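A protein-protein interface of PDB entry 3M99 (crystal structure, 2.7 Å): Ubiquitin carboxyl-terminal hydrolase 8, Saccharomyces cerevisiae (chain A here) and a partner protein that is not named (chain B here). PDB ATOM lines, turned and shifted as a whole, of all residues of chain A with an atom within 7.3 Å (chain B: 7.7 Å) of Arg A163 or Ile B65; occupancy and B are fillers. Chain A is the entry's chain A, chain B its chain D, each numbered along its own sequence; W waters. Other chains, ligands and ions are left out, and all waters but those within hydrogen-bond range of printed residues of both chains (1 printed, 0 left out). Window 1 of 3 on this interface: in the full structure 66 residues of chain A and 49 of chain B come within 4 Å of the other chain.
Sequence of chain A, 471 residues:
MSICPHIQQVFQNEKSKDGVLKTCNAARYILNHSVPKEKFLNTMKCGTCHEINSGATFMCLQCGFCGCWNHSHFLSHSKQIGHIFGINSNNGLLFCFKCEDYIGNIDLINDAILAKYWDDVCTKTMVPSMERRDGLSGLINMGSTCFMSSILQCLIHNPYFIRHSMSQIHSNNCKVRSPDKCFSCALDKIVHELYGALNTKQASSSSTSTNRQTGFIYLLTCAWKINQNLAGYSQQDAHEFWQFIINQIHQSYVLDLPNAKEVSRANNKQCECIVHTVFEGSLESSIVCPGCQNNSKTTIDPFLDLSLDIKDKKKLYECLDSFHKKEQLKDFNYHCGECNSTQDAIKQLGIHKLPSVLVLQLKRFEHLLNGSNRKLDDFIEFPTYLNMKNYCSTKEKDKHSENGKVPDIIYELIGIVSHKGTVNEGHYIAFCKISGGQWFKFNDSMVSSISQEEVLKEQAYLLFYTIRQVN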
ATOM      1  N   ASN A 158      16.878 -11.024  36.100  1.00  0.00           N
ATOM      2  CA  ASN A 158      16.174 -10.729  34.868  1.00  0.00           C
ATOM      3  C   ASN A 158      16.025 -12.004  34.046  1.00  0.00           C
ATOM      4  O   ASN A 158      17.020 -12.666  33.747  1.00  0.00           O
ATOM      5  CB  ASN A 158      16.974  -9.694  34.084  1.00  0.00           C
ATOM      6  CG  ASN A 158      16.135  -8.941  33.076  1.00  0.00           C
ATOM      7  OD1 ASN A 158      16.348  -9.057  31.869  1.00  0.00           O
ATOM      8  ND2 ASN A 158      15.181  -8.154  33.566  1.00  0.00           N
ATOM      9  N   PRO A 159      14.776 -12.353  33.687  1.00  0.00           N
ATOM     10  CA  PRO A 159      14.361 -13.574  32.976  1.00  0.00           C
ATOM     11  C   PRO A 159      15.200 -13.851  31.738  1.00  0.00           C
ATOM     12  O   PRO A 159      15.732 -14.948  31.593  1.00  0.00           O
ATOM     13  CB  PRO A 159      12.920 -13.265  32.574  1.00  0.00           C
ATOM     14  CG  PRO A 159      12.445 -12.320  33.618  1.00  0.00           C
ATOM     15  CD  PRO A 159      13.632 -11.466  33.963  1.00  0.00           C
ATOM     16  N   TYR A 160      15.321 -12.860  30.863  1.00  0.00           N
ATOM     17  CA  TYR A 160      16.170 -12.978  29.685  1.00  0.00           C
ATOM     18  C   TYR A 160      17.635 -13.194  30.021  1.00  0.00           C
ATOM     19  O   TYR A 160      18.281 -14.049  29.415  1.00  0.00           O
ATOM     20  CB  TYR A 160      15.999 -11.772  28.760  1.00  0.00           C
ATOM     21  CG  TYR A 160      14.595 -11.673  28.242  1.00  0.00           C
ATOM     22  CD1 TYR A 160      13.598 -11.087  29.004  1.00  0.00           C
ATOM     23  CD2 TYR A 160      14.250 -12.211  27.015  1.00  0.00           C
ATOM     24  CE1 TYR A 160      12.299 -11.013  28.545  1.00  0.00           C
ATOM     25  CE2 TYR A 160      12.957 -12.142  26.548  1.00  0.00           C
ATOM     26  CZ  TYR A 160      11.986 -11.540  27.317  1.00  0.00           C
ATOM     27  OH  TYR A 160      10.695 -11.460  26.861  1.00  0.00           O
ATOM     28  N   PHE A 161      18.176 -12.442  30.975  1.00  0.00           N
ATOM     29  CA  PHE A 161      19.596 -12.613  31.251  1.00  0.00           C
ATOM     30  C   PHE A 161      19.931 -13.954  31.909  1.00  0.00           C
ATOM     31  O   PHE A 161      20.939 -14.572  31.563  1.00  0.00           O
ATOM     32  CB  PHE A 161      20.216 -11.451  32.029  1.00  0.00           C
ATOM     33  CG  PHE A 161      21.683 -11.633  32.256  1.00  0.00           C
ATOM     34  CD1 PHE A 161      22.604 -11.247  31.294  1.00  0.00           C
ATOM     35  CD2 PHE A 161      22.140 -12.256  33.398  1.00  0.00           C
ATOM     36  CE1 PHE A 161      23.962 -11.449  31.487  1.00  0.00           C
ATOM     37  CE2 PHE A 161      23.484 -12.462  33.592  1.00  0.00           C
ATOM     38  CZ  PHE A 161      24.399 -12.055  32.635  1.00  0.00           C
ATOM     39  N   ILE A 162      19.095 -14.402  32.849  1.00  0.00           N
ATOM     40  CA  ILE A 162      19.265 -15.718  33.468  1.00  0.00           C
ATOM     41  C   ILE A 162      19.242 -16.822  32.420  1.00  0.00           C
ATOM     42  O   ILE A 162      20.076 -17.728  32.431  1.00  0.00           O
ATOM     43  CB  ILE A 162      18.168 -16.024  34.513  1.00  0.00           C
ATOM     44  CG1 ILE A 162      18.098 -14.912  35.538  1.00  0.00           C
ATOM     45  CG2 ILE A 162      18.500 -17.290  35.265  1.00  0.00           C
ATOM     46  CD1 ILE A 162      19.333 -14.859  36.372  1.00  0.00           C
ATOM     47  N   ARG A 163      18.275 -16.745  31.514  1.00  0.00           N
ATOM     48  CA  ARG A 163      18.160 -17.742  30.462  1.00  0.00           C
ATOM     49  C   ARG A 163      19.441 -17.741  29.654  1.00  0.00           C
ATOM     50  O   ARG A 163      20.011 -18.794  29.372  1.00  0.00           O
ATOM     51  CB  ARG A 163      16.962 -17.459  29.561  1.00  0.00           C
ATOM     52  CG  ARG A 163      16.677 -18.568  28.572  1.00  0.00           C
ATOM     53  CD  ARG A 163      15.341 -18.375  27.883  1.00  0.00           C
ATOM     54  NE  ARG A 163      15.420 -17.483  26.728  1.00  0.00           N
ATOM     55  CZ  ARG A 163      14.501 -17.427  25.766  1.00  0.00           C
ATOM     56  NH1 ARG A 163      13.434 -18.216  25.821  1.00  0.00           N
ATOM     57  NH2 ARG A 163      14.645 -16.589  24.750  1.00  0.00           N
ATOM     58  N   HIS A 164      19.905 -16.548  29.302  1.00  0.00           N
ATOM     59  CA  HIS A 164      21.119 -16.423  28.509  1.00  0.00           C
ATOM     60  C   HIS A 164      22.328 -17.041  29.204  1.00  0.00           C
ATOM     61  O   HIS A 164      23.020 -17.874  28.621  1.00  0.00           O
ATOM     62  CB  HIS A 164      21.391 -14.963  28.132  1.00  0.00           C
ATOM     63  CG  HIS A 164      22.701 -14.762  27.442  1.00  0.00           C
ATOM     64  ND1 HIS A 164      22.917 -15.121  26.129  1.00  0.00           N
ATOM     65  CD2 HIS A 164      23.876 -14.251  27.889  1.00  0.00           C
ATOM     66  CE1 HIS A 164      24.164 -14.837  25.794  1.00  0.00           C
ATOM     67  NE2 HIS A 164      24.765 -14.306  26.845  1.00  0.00           N
ATOM     68  N   SER A 165      22.572 -16.643  30.451  1.00  0.00           N
ATOM     69  CA  SER A 165      23.702 -17.170  31.217  1.00  0.00           C
ATOM     70  C   SER A 165      23.657 -18.690  31.398  1.00  0.00           C
ATOM     71  O   SER A 165      24.643 -19.371  31.125  1.00  0.00           O
ATOM     72  CB  SER A 165      23.813 -16.482  32.583  1.00  0.00           C
ATOM     73  OG  SER A 165      24.830 -17.083  33.372  1.00  0.00           O
ATOM     74  N   MET A 166      22.518 -19.215  31.855  1.00  0.00           N
ATOM     75  CA  MET A 166      22.395 -20.651  32.143  1.00  0.00           C
ATOM     76  C   MET A 166      22.385 -21.520  30.882  1.00  0.00           C
ATOM     77  O   MET A 166      22.723 -22.701  30.932  1.00  0.00           O
ATOM     78  CB  MET A 166      21.183 -20.953  33.038  1.00  0.00           C
ATOM     79  CG  MET A 166      21.357 -20.489  34.480  1.00  0.00           C
ATOM     80  SD  MET A 166      19.946 -20.871  35.534  1.00  0.00           S
ATOM     81  CE  MET A 166      18.650 -20.880  34.293  1.00  0.00           C
ATOM     82  N   SER A 167      22.019 -20.932  29.751  1.00  0.00           N
ATOM     83  CA  SER A 167      22.119 -21.636  28.483  1.00  0.00           C
ATOM     84  C   SER A 167      23.584 -21.835  28.094  1.00  0.00           C
ATOM     85  O   SER A 167      23.886 -22.473  27.083  1.00  0.00           O
ATOM     86  CB  SER A 167      21.376 -20.873  27.388  1.00  0.00           C
ATOM     87  OG  SER A 167      19.977 -21.100  27.459  1.00  0.00           O
ATOM     88  N   GLN A 168      24.484 -21.286  28.911  1.00  0.00           N
ATOM     89  CA  GLN A 168      25.929 -21.306  28.655  1.00  0.00           C
ATOM     90  C   GLN A 168      26.305 -20.728  27.280  1.00  0.00           C
ATOM     91  O   GLN A 168      27.398 -20.973  26.764  1.00  0.00           O
ATOM     92  CB  GLN A 168      26.500 -22.716  28.831  1.00  0.00           C
ATOM     93  CG  GLN A 168      26.077 -23.411  30.117  1.00  0.00           C
ATOM     94  CD  GLN A 168      26.505 -22.663  31.366  1.00  0.00           C
ATOM     95  OE1 GLN A 168      27.644 -22.210  31.480  1.00  0.00           O
ATOM     96  NE2 GLN A 168      25.590 -22.537  32.318  1.00  0.00           N
ATOM     97  N   ILE A 169      25.397 -19.945  26.705  1.00  0.00           N
ATOM     98  CA  ILE A 169      25.583 -19.378  25.373  1.00  0.00           C
ATOM     99  C   ILE A 169      26.927 -18.687  25.212  1.00  0.00           C
ATOM    100  O   ILE A 169      27.599 -18.842  24.193  1.00  0.00           O
ATOM    101  CB  ILE A 169      24.492 -18.351  25.049  1.00  0.00           C
ATOM    102  CG1 ILE A 169      23.100 -18.977  25.201  1.00  0.00           C
ATOM    103  CG2 ILE A 169      24.700 -17.788  23.659  1.00  0.00           C
ATOM    104  CD1 ILE A 169      22.902 -20.247  24.418  1.00  0.00           C
ATOM    105  N   ILE A 274      22.332 -10.723  23.176  1.00  0.00           N
ATOM    106  CA  ILE A 274      21.134 -10.584  24.000  1.00  0.00           C
ATOM    107  C   ILE A 274      20.731  -9.138  24.191  1.00  0.00           C
ATOM    108  O   ILE A 274      19.548  -8.810  24.181  1.00  0.00           O
ATOM    109  CB  ILE A 274      21.309 -11.187  25.396  1.00  0.00           C
ATOM    110  CG1 ILE A 274      22.467 -12.184  25.410  1.00  0.00           C
ATOM    111  CG2 ILE A 274      20.005 -11.816  25.858  1.00  0.00           C
ATOM    112  CD1 ILE A 274      23.842 -11.527  25.374  1.00  0.00           C
ATOM    113  N   VAL A 278      17.179  -7.949  23.290  1.00  0.00           N
ATOM    114  CA  VAL A 278      16.286  -7.810  24.435  1.00  0.00           C
ATOM    115  C   VAL A 278      15.981  -6.356  24.832  1.00  0.00           C
ATOM    116  O   VAL A 278      14.815  -5.981  25.017  1.00  0.00           O
ATOM    117  CB  VAL A 278      16.844  -8.589  25.648  1.00  0.00           C
ATOM    118  CG1 VAL A 278      16.150  -8.174  26.933  1.00  0.00           C
ATOM    119  CG2 VAL A 278      16.708 -10.089  25.415  1.00  0.00           C
ATOM    120  N   SER A 356      12.082  -5.984  24.437  1.00  0.00           N
ATOM    121  CA  SER A 356      11.490  -7.037  25.257  1.00  0.00           C
ATOM    122  C   SER A 356      11.469  -6.564  26.704  1.00  0.00           C
ATOM    123  O   SER A 356      10.437  -6.601  27.368  1.00  0.00           O
ATOM    124  CB  SER A 356      12.280  -8.337  25.121  1.00  0.00           C
ATOM    125  OG  SER A 356      12.449  -8.681  23.758  1.00  0.00           O
ATOM    126  N   THR A 466       9.419  -6.105  31.821  1.00  0.00           N
ATOM    127  CA  THR A 466       9.468  -7.124  30.772  1.00  0.00           C
ATOM    128  C   THR A 466       8.127  -7.219  30.075  1.00  0.00           C
ATOM    129  O   THR A 466       7.080  -7.051  30.694  1.00  0.00           O
ATOM    130  CB  THR A 466       9.864  -8.524  31.282  1.00  0.00           C
ATOM    131  OG1 THR A 466       9.179  -8.807  32.506  1.00  0.00           O
ATOM    132  CG2 THR A 466      11.350  -8.609  31.514  1.00  0.00           C
ATOM    133  N   ILE A 467       8.168  -7.483  28.778  1.00  0.00           N
ATOM    134  CA  ILE A 467       6.957  -7.512  27.971  1.00  0.00           C
ATOM    135  C   ILE A 467       6.098  -8.677  28.426  1.00  0.00           C
ATOM    136  O   ILE A 467       6.617  -9.726  28.813  1.00  0.00           O
ATOM    137  CB  ILE A 467       7.289  -7.599  26.456  1.00  0.00           C
ATOM    138  CG1 ILE A 467       6.037  -7.371  25.605  1.00  0.00           C
ATOM    139  CG2 ILE A 467       7.984  -8.905  26.131  1.00  0.00           C
ATOM    140  CD1 ILE A 467       5.350  -6.055  25.899  1.00  0.00           C
ATOM    141  N   ARG A 468       4.783  -8.499  28.412  1.00  0.00           N
ATOM    142  CA  ARG A 468       3.933  -9.582  28.881  1.00  0.00           C
ATOM    143  C   ARG A 468       2.728  -9.914  28.005  1.00  0.00           C
ATOM    144  O   ARG A 468       2.482 -11.088  27.713  1.00  0.00           O
ATOM    145  CB  ARG A 468       3.530  -9.392  30.335  1.00  0.00           C
ATOM    146  CG  ARG A 468       3.328 -10.723  30.990  1.00  0.00           C
ATOM    147  CD  ARG A 468       2.501 -10.627  32.218  1.00  0.00           C
ATOM    148  NE  ARG A 468       1.665 -11.810  32.353  1.00  0.00           N
ATOM    149  CZ  ARG A 468       0.956 -12.090  33.436  1.00  0.00           C
ATOM    150  NH1 ARG A 468       0.999 -11.273  34.480  1.00  0.00           N
ATOM    151  NH2 ARG A 468       0.215 -13.190  33.473  1.00  0.00           N
ATOM    152  N   LEU B  44       7.113 -21.004  16.100  1.00  0.00           N
ATOM    153  CA  LEU B  44       6.716 -20.769  17.482  1.00  0.00           C
ATOM    154  C   LEU B  44       5.660 -19.675  17.613  1.00  0.00           C
ATOM    155  O   LEU B  44       5.800 -18.589  17.058  1.00  0.00           O
ATOM    156  CB  LEU B  44       7.940 -20.412  18.317  1.00  0.00           C
ATOM    157  CG  LEU B  44       7.787 -20.466  19.834  1.00  0.00           C
ATOM    158  CD1 LEU B  44       7.666 -21.901  20.291  1.00  0.00           C
ATOM    159  CD2 LEU B  44       8.979 -19.800  20.500  1.00  0.00           C
ATOM    160  N   TYR B  46       2.599 -17.642  20.298  1.00  0.00           N
ATOM    161  CA  TYR B  46       2.334 -17.306  21.704  1.00  0.00           C
ATOM    162  C   TYR B  46       0.838 -17.067  21.955  1.00  0.00           C
ATOM    163  O   TYR B  46       0.125 -16.565  21.085  1.00  0.00           O
ATOM    164  CB  TYR B  46       3.170 -16.097  22.164  1.00  0.00           C
ATOM    165  CG  TYR B  46       4.633 -16.160  21.758  1.00  0.00           C
ATOM    166  CD1 TYR B  46       5.062 -15.629  20.546  1.00  0.00           C
ATOM    167  CD2 TYR B  46       5.583 -16.754  22.579  1.00  0.00           C
ATOM    168  CE1 TYR B  46       6.390 -15.694  20.164  1.00  0.00           C
ATOM    169  CE2 TYR B  46       6.918 -16.819  22.203  1.00  0.00           C
ATOM    170  CZ  TYR B  46       7.311 -16.289  20.993  1.00  0.00           C
ATOM    171  OH  TYR B  46       8.627 -16.350  20.604  1.00  0.00           O
ATOM    172  N   HIS B  48      -0.567 -15.070  24.265  1.00  0.00           N
ATOM    173  CA  HIS B  48      -0.860 -13.672  24.547  1.00  0.00           C
ATOM    174  C   HIS B  48      -0.266 -12.754  23.488  1.00  0.00           C
ATOM    175  O   HIS B  48      -0.961 -11.922  22.909  1.00  0.00           O
ATOM    176  CB  HIS B  48      -0.309 -13.296  25.916  1.00  0.00           C
ATOM    177  CG  HIS B  48      -0.481 -14.364  26.945  1.00  0.00           C
ATOM    178  ND1 HIS B  48      -1.721 -14.815  27.345  1.00  0.00           N
ATOM    179  CD2 HIS B  48       0.425 -15.068  27.662  1.00  0.00           C
ATOM    180  CE1 HIS B  48      -1.570 -15.750  28.266  1.00  0.00           C
ATOM    181  NE2 HIS B  48      -0.276 -15.921  28.477  1.00  0.00           N
ATOM    182  N   MET B  49       1.029 -12.905  23.240  1.00  0.00           N
ATOM    183  CA  MET B  49       1.704 -12.078  22.256  1.00  0.00           C
ATOM    184  C   MET B  49       1.252 -12.407  20.834  1.00  0.00           C
ATOM    185  O   MET B  49       1.578 -13.470  20.302  1.00  0.00           O
ATOM    186  CB  MET B  49       3.220 -12.228  22.393  1.00  0.00           C
ATOM    187  CG  MET B  49       3.866 -11.180  23.287  1.00  0.00           C
ATOM    188  SD  MET B  49       4.466 -11.796  24.862  1.00  0.00           S
ATOM    189  CE  MET B  49       5.751 -12.914  24.320  1.00  0.00           C
ATOM    190  N   ALA B  62      13.771 -10.190  17.800  1.00  0.00           N
ATOM    191  CA  ALA B  62      13.410 -10.111  19.217  1.00  0.00           C
ATOM    192  C   ALA B  62      13.482 -11.440  19.963  1.00  0.00           C
ATOM    193  O   ALA B  62      12.927 -12.443  19.519  1.00  0.00           O
ATOM    194  CB  ALA B  62      12.017  -9.521  19.359  1.00  0.00           C
ATOM    195  N   GLN B  63      14.158 -11.438  21.106  1.00  0.00           N
ATOM    196  CA  GLN B  63      14.187 -12.594  21.993  1.00  0.00           C
ATOM    197  C   GLN B  63      12.963 -12.533  22.893  1.00  0.00           C
ATOM    198  O   GLN B  63      12.746 -11.540  23.574  1.00  0.00           O
ATOM    199  CB  GLN B  63      15.458 -12.578  22.837  1.00  0.00           C
ATOM    200  CG  GLN B  63      15.668 -13.807  23.692  1.00  0.00           C
ATOM    201  CD  GLN B  63      17.081 -13.893  24.253  1.00  0.00           C
ATOM    202  OE1 GLN B  63      18.062 -13.706  23.529  1.00  0.00           O
ATOM    203  NE2 GLN B  63      17.189 -14.189  25.550  1.00  0.00           N
ATOM    204  N   LEU B  64      12.161 -13.593  22.903  1.00  0.00           N
ATOM    205  CA  LEU B  64      10.918 -13.579  23.680  1.00  0.00           C
ATOM    206  C   LEU B  64      10.735 -14.681  24.738  1.00  0.00           C
ATOM    207  O   LEU B  64      11.243 -15.795  24.603  1.00  0.00           O
ATOM    208  CB  LEU B  64       9.710 -13.545  22.746  1.00  0.00           C
ATOM    209  CG  LEU B  64       9.442 -12.145  22.207  1.00  0.00           C
ATOM    210  CD1 LEU B  64       8.095 -12.085  21.519  1.00  0.00           C
ATOM    211  CD2 LEU B  64       9.494 -11.175  23.359  1.00  0.00           C
ATOM    212  N   ILE B  65      10.003 -14.330  25.794  1.00  0.00           N
ATOM    213  CA  ILE B  65       9.629 -15.237  26.870  1.00  0.00           C
ATOM    214  C   ILE B  65       8.178 -14.932  27.217  1.00  0.00           C
ATOM    215  O   ILE B  65       7.860 -13.796  27.568  1.00  0.00           O
ATOM    216  CB  ILE B  65      10.442 -14.985  28.145  1.00  0.00           C
ATOM    217  CG1 ILE B  65      11.939 -15.087  27.882  1.00  0.00           C
ATOM    218  CG2 ILE B  65      10.060 -15.995  29.198  1.00  0.00           C
ATOM    219  CD1 ILE B  65      12.473 -16.468  28.075  1.00  0.00           C
ATOM    220  N   GLU B  66       7.297 -15.928  27.126  1.00  0.00           N
ATOM    221  CA  GLU B  66       5.864 -15.691  27.335  1.00  0.00           C
ATOM    222  C   GLU B  66       5.567 -14.966  28.644  1.00  0.00           C
ATOM    223  O   GLU B  66       5.336 -13.757  28.660  1.00  0.00           O
ATOM    224  CB  GLU B  66       5.073 -16.997  27.264  1.00  0.00           C
ATOM    225  CG  GLU B  66       4.491 -17.311  25.885  1.00  0.00           C
ATOM    226  CD  GLU B  66       3.075 -16.772  25.695  1.00  0.00           C
ATOM    227  OE1 GLU B  66       2.825 -15.587  26.008  1.00  0.00           O
ATOM    228  OE2 GLU B  66       2.210 -17.541  25.227  1.00  0.00           O
ATOM    229  N   ASP B  67       5.560 -15.712  29.737  1.00  0.00           N
ATOM    230  CA  ASP B  67       5.317 -15.138  31.047  1.00  0.00           C
ATOM    231  C   ASP B  67       6.529 -15.469  31.886  1.00  0.00           C
ATOM    232  O   ASP B  67       6.584 -16.523  32.509  1.00  0.00           O
ATOM    233  CB  ASP B  67       4.057 -15.750  31.656  1.00  0.00           C
ATOM    234  CG  ASP B  67       2.821 -15.489  30.814  1.00  0.00           C
ATOM    235  OD1 ASP B  67       1.793 -16.179  30.995  1.00  0.00           O
ATOM    236  OD2 ASP B  67       2.878 -14.586  29.956  1.00  0.00           O
ATOM    237  N   PRO B  68       7.517 -14.574  31.888  1.00  0.00           N
ATOM    238  CA  PRO B  68       8.845 -14.848  32.438  1.00  0.00           C
ATOM    239  C   PRO B  68       8.751 -15.228  33.905  1.00  0.00           C
ATOM    240  O   PRO B  68       9.492 -16.092  34.375  1.00  0.00           O
ATOM    241  CB  PRO B  68       9.562 -13.506  32.266  1.00  0.00           C
ATOM    242  CG  PRO B  68       8.446 -12.507  32.207  1.00  0.00           C
ATOM    243  CD  PRO B  68       7.412 -13.192  31.401  1.00  0.00           C
ATOM    244  N   LEU B  69       7.840 -14.578  34.619  1.00  0.00           N
ATOM    245  CA  LEU B  69       7.578 -14.917  36.007  1.00  0.00           C
ATOM    246  C   LEU B  69       6.285 -15.696  36.063  1.00  0.00           C
ATOM    247  O   LEU B  69       5.272 -15.187  36.540  1.00  0.00           O
ATOM    248  CB  LEU B  69       7.405 -13.663  36.863  1.00  0.00           C
ATOM    249  CG  LEU B  69       8.402 -12.508  36.829  1.00  0.00           C
ATOM    250  CD1 LEU B  69       8.181 -11.668  38.077  1.00  0.00           C
ATOM    251  CD2 LEU B  69       9.847 -12.989  36.748  1.00  0.00           C
ATOM    252  N   ASP B  70       6.298 -16.916  35.546  1.00  0.00           N
ATOM    253  CA  ASP B  70       5.131 -17.771  35.653  1.00  0.00           C
ATOM    254  C   ASP B  70       5.445 -18.778  36.730  1.00  0.00           C
ATOM    255  O   ASP B  70       4.717 -18.923  37.709  1.00  0.00           O
ATOM    256  CB  ASP B  70       4.871 -18.495  34.336  1.00  0.00           C
ATOM    257  CG  ASP B  70       3.865 -19.614  34.487  1.00  0.00           C
ATOM    258  OD1 ASP B  70       2.939 -19.451  35.315  1.00  0.00           O
ATOM    259  OD2 ASP B  70       4.004 -20.651  33.791  1.00  0.00           O
ATOM    260  N   ILE B  73      12.543 -20.312  37.895  1.00  0.00           N
ATOM    261  CA  ILE B  73      13.429 -20.654  36.798  1.00  0.00           C
ATOM    262  C   ILE B  73      13.749 -22.147  36.865  1.00  0.00           C
ATOM    263  O   ILE B  73      14.055 -22.683  37.928  1.00  0.00           O
ATOM    264  CB  ILE B  73      14.697 -19.763  36.815  1.00  0.00           C
ATOM    265  CG1 ILE B  73      15.767 -20.315  35.881  1.00  0.00           C
ATOM    266  CG2 ILE B  73      15.217 -19.596  38.230  1.00  0.00           C
ATOM    267  CD1 ILE B  73      15.331 -20.345  34.430  1.00  0.00           C
ATOM    268  N   PRO B  84      24.940 -23.741  37.190  1.00  0.00           N
ATOM    269  CA  PRO B  84      23.495 -23.871  36.970  1.00  0.00           C
ATOM    270  C   PRO B  84      23.175 -23.964  35.478  1.00  0.00           C
ATOM    271  O   PRO B  84      23.225 -22.955  34.773  1.00  0.00           O
ATOM    272  CB  PRO B  84      22.932 -22.563  37.541  1.00  0.00           C
ATOM    273  CG  PRO B  84      24.063 -21.919  38.282  1.00  0.00           C
ATOM    274  CD  PRO B  84      25.304 -22.383  37.613  1.00  0.00           C
ATOM    275  N   LEU B  85      22.849 -25.166  35.015  1.00  0.00           N
ATOM    276  CA  LEU B  85      22.575 -25.419  33.608  1.00  0.00           C
ATOM    277  C   LEU B  85      21.122 -25.167  33.270  1.00  0.00           C
ATOM    278  O   LEU B  85      20.233 -25.488  34.052  1.00  0.00           O
ATOM    279  CB  LEU B  85      22.907 -26.868  33.260  1.00  0.00           C
ATOM    280  CG  LEU B  85      24.268 -27.387  33.716  1.00  0.00           C
ATOM    281  CD1 LEU B  85      24.384 -28.882  33.483  1.00  0.00           C
ATOM    282  CD2 LEU B  85      25.374 -26.649  32.993  1.00  0.00           C
ATOM    283  N   ALA B  86      20.886 -24.598  32.093  1.00  0.00           N
ATOM    284  CA  ALA B  86      19.536 -24.425  31.585  1.00  0.00           C
ATOM    285  C   ALA B  86      18.965 -25.792  31.253  1.00  0.00           C
ATOM    286  O   ALA B  86      19.701 -26.740  30.964  1.00  0.00           O
ATOM    287  CB  ALA B  86      19.528 -23.527  30.360  1.00  0.00           C
ATOM    288  N   THR B  88      18.038 -27.017  28.901  1.00  0.00           N
ATOM    289  CA  THR B  88      18.123 -27.183  27.451  1.00  0.00           C
ATOM    290  C   THR B  88      19.581 -27.098  26.988  1.00  0.00           C
ATOM    291  O   THR B  88      19.881 -27.190  25.800  1.00  0.00           O
ATOM    292  CB  THR B  88      17.297 -26.086  26.736  1.00  0.00           C
ATOM    293  OG1 THR B  88      16.978 -26.489  25.399  1.00  0.00           O
ATOM    294  CG2 THR B  88      18.065 -24.777  26.703  1.00  0.00           C
ATOM    295  N   ALA B  89      20.483 -26.916  27.947  1.00  0.00           N
ATOM    296  CA  ALA B  89      21.906 -26.780  27.678  1.00  0.00           C
ATOM    297  C   ALA B  89      22.644 -27.864  28.441  1.00  0.00           C
ATOM    298  O   ALA B  89      23.868 -27.979  28.343  1.00  0.00           O
ATOM    299  CB  ALA B  89      22.388 -25.407  28.115  1.00  0.00           C
HETATM  300  O   HOH W   1       8.974 -11.342  28.751  1.00  0.00           O
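O of Arg A163 lies within hydrogen-bond range of OG of Ser A167, at 3.0 Å. The backbone carbonyl oxygen (O) of Val A278 lies within hydrogen-bond range of the backbone NH (N) of Ser A356 (2.8 Å). OD1 of Asp B67 is in hydrogen-bond range of NE2 of His B48.
Among the printed residues, pairs that only touch across the chains: Pro A159 with Pro B68 (3.4 Å), Tyr A160 with Gln B63 (3.0 Å), Tyr A160 with Leu B64 (3.7 Å), Arg A163 with Gln B63 (3.1 Å), Arg A163 with Ile B65 (3.0 Å), Met A166 with Ile B73 (3.3 Å), Met A166 with Pro B84 (3.1 Å), Met A166 with Leu B85 (3.8 Å), Met A166 with Ala B89 (3.9 Å), Ser A167 with Ala B86 (3.6 Å), Ser A167 with Ala B89 (3.5 Å), Ile A274 with Gln B63 (3.6 Å), Val A278 with Gln B63 (3.8 Å), Ser A356 with Leu B64 (3.9 Å), Thr A466 with Pro B68 (3.8 Å), Ile A467 with Leu B64 (3.9 Å) and Arg A468 with His B48 (3.99 Å).
Arg A163 touches just these residues of chain B: Gln B63 (3.1 Å), Leu B64 (3.5 Å) and Ile B65 (3.0 Å). Of chain A, only Tyr A160 (3.1 Å) and Arg A163 (3.0 Å) come within 4 Å of Ile B65. Of the printed residues of chain B, Ile A467 touches Leu B64. Printed residues of chain A within 4 Å of Ala B89: Met A166 (3.9 Å) and Ser A167 (3.5 Å). Ser A165 touches none of the printed residues of chain B. Ala B62 touches none of the printed residues of chain A.
Printed residues of chain A that touch a printed residue of chain B: Pro A159, Tyr A160, Arg A163, Met A166, Ser A167, Gln A168, Ile A274, Val A278, Ser A356, Thr A466, Ile A467 and Arg A468. Hydrophobic or aromatic side chains of chain A within 4 Å of the printed part of chain B: Pro A159, Tyr A160, Met A166, Ile A274, Val A278 and Ile A467. Along chain A the printed residues that touch a printed residue of chain B span positions 159 to 468. Among the printed residues, Asp or Glu carboxylates within 4 Å of a Lys or Arg side-chain nitrogen of the other chain: Arg A468 with Asp B67.
The side-chain hydroxyl of Tyr A160 sits at hydrogen-bond distance from the backbone NH of Ile B65, 3.1 Å away. The guanidinium group (NH1) of Arg A163 sits at hydrogen-bond distance from the backbone carbonyl oxygen (O) of Leu B64 (3.5 Å). N of Ala B86 sits at hydrogen-bond distance from O of Met A166 (2.9 Å). NE2 of Gln A168 is in hydrogen-bond range of O of Pro B84, at 3.4 Å. OG of Ser A356 sits at hydrogen-bond distance from O of Gln B63. The guanidinium group of Arg A468 lies within salt-bridge range of the side-chain carboxylate of Asp B67 (3.9 Å). The backbone carbonyl oxygen (O) of Arg A468 sits close to the side-chain sulfur (SD) of Met B49 (3.5 Å).
Water W1 lies within hydrogen-bond range of the side-chain hydroxyl of Tyr A160 (2.6 Å), the backbone carbonyl oxygen of Ile A467 (2.9 Å) and the backbone carbonyl oxygen of Ile B65 (2.9 Å).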
